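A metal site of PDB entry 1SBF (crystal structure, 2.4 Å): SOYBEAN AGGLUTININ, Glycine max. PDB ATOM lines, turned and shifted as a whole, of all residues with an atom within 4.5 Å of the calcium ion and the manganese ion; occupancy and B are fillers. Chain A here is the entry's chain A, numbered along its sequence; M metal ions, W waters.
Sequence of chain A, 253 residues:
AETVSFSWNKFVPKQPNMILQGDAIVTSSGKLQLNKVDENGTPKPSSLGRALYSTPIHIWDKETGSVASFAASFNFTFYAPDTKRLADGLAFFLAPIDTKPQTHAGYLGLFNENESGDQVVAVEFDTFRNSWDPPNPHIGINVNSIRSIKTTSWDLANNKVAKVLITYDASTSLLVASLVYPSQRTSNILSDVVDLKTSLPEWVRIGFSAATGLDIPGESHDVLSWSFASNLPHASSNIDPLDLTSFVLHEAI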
ATOM      1  N   GLU A 124      18.318 -31.372 -23.197  1.00  0.00           N
ATOM      2  CA  GLU A 124      19.428 -32.073 -23.843  1.00  0.00           C
ATOM      3  C   GLU A 124      20.116 -33.104 -22.998  1.00  0.00           C
ATOM      4  O   GLU A 124      20.257 -32.957 -21.791  1.00  0.00           O
ATOM      5  CB  GLU A 124      20.482 -31.037 -24.301  1.00  0.00           C
ATOM      6  CG  GLU A 124      21.422 -30.563 -23.163  1.00  0.00           C
ATOM      7  CD  GLU A 124      22.618 -29.775 -23.650  1.00  0.00           C
ATOM      8  OE1 GLU A 124      22.372 -29.098 -24.741  1.00  0.00           O
ATOM      9  OE2 GLU A 124      23.738 -29.868 -23.187  1.00  0.00           O
ATOM     10  N   ASP A 126      23.742 -34.269 -23.335  1.00  0.00           N
ATOM     11  CA  ASP A 126      24.871 -33.840 -24.129  1.00  0.00           C
ATOM     12  C   ASP A 126      26.168 -34.590 -23.832  1.00  0.00           C
ATOM     13  O   ASP A 126      26.678 -34.522 -22.719  1.00  0.00           O
ATOM     14  CB  ASP A 126      24.994 -32.307 -23.947  1.00  0.00           C
ATOM     15  CG  ASP A 126      26.108 -31.755 -24.772  1.00  0.00           C
ATOM     16  OD1 ASP A 126      26.895 -32.459 -25.370  1.00  0.00           O
ATOM     17  OD2 ASP A 126      25.994 -30.465 -24.957  1.00  0.00           O
ATOM     18  N   PHE A 128      29.177 -34.334 -25.695  1.00  0.00           N
ATOM     19  CA  PHE A 128      30.389 -33.743 -26.152  1.00  0.00           C
ATOM     20  C   PHE A 128      30.545 -32.305 -25.722  1.00  0.00           C
ATOM     21  O   PHE A 128      29.654 -31.484 -25.940  1.00  0.00           O
ATOM     22  CB  PHE A 128      30.445 -33.848 -27.661  1.00  0.00           C
ATOM     23  CG  PHE A 128      31.807 -33.430 -28.101  1.00  0.00           C
ATOM     24  CD1 PHE A 128      32.875 -34.318 -27.998  1.00  0.00           C
ATOM     25  CD2 PHE A 128      32.066 -32.109 -28.464  1.00  0.00           C
ATOM     26  CE1 PHE A 128      34.154 -33.955 -28.400  1.00  0.00           C
ATOM     27  CE2 PHE A 128      33.333 -31.706 -28.856  1.00  0.00           C
ATOM     28  CZ  PHE A 128      34.382 -32.631 -28.813  1.00  0.00           C
ATOM     29  N   ARG A 129      31.690 -32.005 -25.112  1.00  0.00           N
ATOM     30  CA  ARG A 129      31.991 -30.652 -24.629  1.00  0.00           C
ATOM     31  C   ARG A 129      32.293 -29.688 -25.756  1.00  0.00           C
ATOM     32  O   ARG A 129      33.357 -29.741 -26.336  1.00  0.00           O
ATOM     33  CB  ARG A 129      33.154 -30.627 -23.626  1.00  0.00           C
ATOM     34  N   ASN A 130      31.377 -28.762 -26.035  1.00  0.00           N
ATOM     35  CA  ASN A 130      31.682 -27.721 -26.976  1.00  0.00           C
ATOM     36  C   ASN A 130      32.138 -26.543 -26.175  1.00  0.00           C
ATOM     37  O   ASN A 130      32.182 -26.624 -24.943  1.00  0.00           O
ATOM     38  CB  ASN A 130      30.504 -27.405 -27.912  1.00  0.00           C
ATOM     39  CG  ASN A 130      29.942 -28.710 -28.455  1.00  0.00           C
ATOM     40  OD1 ASN A 130      29.107 -29.381 -27.823  1.00  0.00           O
ATOM     41  ND2 ASN A 130      30.552 -29.192 -29.534  1.00  0.00           N
ATOM     42  N   TRP A 132      30.812 -23.854 -25.378  1.00  0.00           N
ATOM     43  CA  TRP A 132      29.819 -23.318 -24.463  1.00  0.00           C
ATOM     44  C   TRP A 132      29.479 -24.245 -23.314  1.00  0.00           C
ATOM     45  O   TRP A 132      28.737 -23.839 -22.419  1.00  0.00           O
ATOM     46  CB  TRP A 132      28.520 -22.950 -25.188  1.00  0.00           C
ATOM     47  CG  TRP A 132      28.000 -24.099 -25.996  1.00  0.00           C
ATOM     48  CD1 TRP A 132      27.229 -25.117 -25.538  1.00  0.00           C
ATOM     49  CD2 TRP A 132      28.305 -24.396 -27.352  1.00  0.00           C
ATOM     50  NE1 TRP A 132      27.011 -26.027 -26.532  1.00  0.00           N
ATOM     51  CE2 TRP A 132      27.639 -25.599 -27.654  1.00  0.00           C
ATOM     52  CE3 TRP A 132      29.029 -23.727 -28.334  1.00  0.00           C
ATOM     53  CZ2 TRP A 132      27.678 -26.145 -28.937  1.00  0.00           C
ATOM     54  CZ3 TRP A 132      29.061 -24.262 -29.604  1.00  0.00           C
ATOM     55  CH2 TRP A 132      28.408 -25.481 -29.887  1.00  0.00           C
ATOM     56  N   ASP A 133      30.031 -25.460 -23.351  1.00  0.00           N
ATOM     57  CA  ASP A 133      29.663 -26.552 -22.462  1.00  0.00           C
ATOM     58  C   ASP A 133      30.450 -26.632 -21.197  1.00  0.00           C
ATOM     59  O   ASP A 133      31.596 -26.193 -21.147  1.00  0.00           O
ATOM     60  CB  ASP A 133      29.786 -27.893 -23.202  1.00  0.00           C
ATOM     61  CG  ASP A 133      28.600 -28.187 -24.077  1.00  0.00           C
ATOM     62  OD1 ASP A 133      27.448 -28.026 -23.454  1.00  0.00           O
ATOM     63  OD2 ASP A 133      28.708 -28.499 -25.251  1.00  0.00           O
ATOM     64  N   HIS A 138      26.259 -34.195 -19.665  1.00  0.00           N
ATOM     65  CA  HIS A 138      25.346 -33.464 -18.821  1.00  0.00           C
ATOM     66  C   HIS A 138      23.969 -33.509 -19.411  1.00  0.00           C
ATOM     67  O   HIS A 138      23.752 -33.941 -20.550  1.00  0.00           O
ATOM     68  CB  HIS A 138      25.824 -31.988 -18.654  1.00  0.00           C
ATOM     69  CG  HIS A 138      26.125 -31.289 -19.968  1.00  0.00           C
ATOM     70  ND1 HIS A 138      27.284 -31.542 -20.703  1.00  0.00           N
ATOM     71  CD2 HIS A 138      25.390 -30.377 -20.679  1.00  0.00           C
ATOM     72  CE1 HIS A 138      27.233 -30.782 -21.796  1.00  0.00           C
ATOM     73  NE2 HIS A 138      26.127 -30.040 -21.802  1.00  0.00           N
ATOM     74  N   SER A 148      23.083 -23.798 -22.685  1.00  0.00           N
ATOM     75  CA  SER A 148      22.096 -24.147 -21.649  1.00  0.00           C
ATOM     76  C   SER A 148      21.938 -23.161 -20.489  1.00  0.00           C
ATOM     77  O   SER A 148      22.927 -22.720 -19.929  1.00  0.00           O
ATOM     78  CB  SER A 148      22.245 -25.578 -21.143  1.00  0.00           C
ATOM     79  OG  SER A 148      22.408 -26.473 -22.232  1.00  0.00           O
HETATM   80 CA    CA M   1      27.790 -30.413 -26.441  1.00  0.00          CA
HETATM   81 MN    MN M   2      25.542 -28.937 -23.663  1.00  0.00          MN
HETATM   82  O   HOH W   1      26.301 -28.900 -27.425  1.00  0.00           O
HETATM   83  O   HOH W   2      24.964 -27.417 -22.520  1.00  0.00           O
HETATM   84  O   HOH W   3      27.650 -31.969 -27.826  1.00  0.00           O
HETATM   85  O   HOH W   4      24.856 -27.903 -25.323  1.00  0.00           O
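Water W4 lies within hydrogen-bond range of the side-chain carboxylate of Glu 124 (2.8 Å) and the indole nitrogen of Trp 132 (3.1 Å).
Of the 9 residues printed, 4 come within 4 Å of the manganese ion.
The side-chain carboxylate (OD2) of Asp 133 sits close to the indole nitrogen (NE1) of Trp 132.
Of the 9 residues printed, 4 come within 4 Å of the calcium ion.
Water W2 binds the manganese ion, 2.0 Å away.
The side-chain carboxylate (OD2) of Asp 126 is bound to the manganese ion (2.1 Å).
Water W4 binds the manganese ion (2.1 Å).
The side-chain carboxylate (OE2) of Glu 124 binds the manganese ion (2.1 Å).
The manganese ion is bound by OD1 of Asp 133, 2.1 Å away.
The manganese ion is bound by NE2 of His 138 (2.2 Å).
The manganese ion has six donor atoms within binding distance.
The calcium ion is bound by water W3 (2.1 Å), the side-chain amide oxygen (OD1) of Asn 130 (2.2 Å), the backbone carbonyl oxygen (O) of Phe 128 (2.2 Å), the side-chain carboxylate (OD2) of Asp 126 (2.3 Å), water W1 (2.3 Å), the side-chain carboxylate (OD2) of Asp 133 (2.4 Å) and the side-chain carboxylate (OD1) of Asp 126 (2.5 Å).
The calcium ion has seven donor atoms within binding distance.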
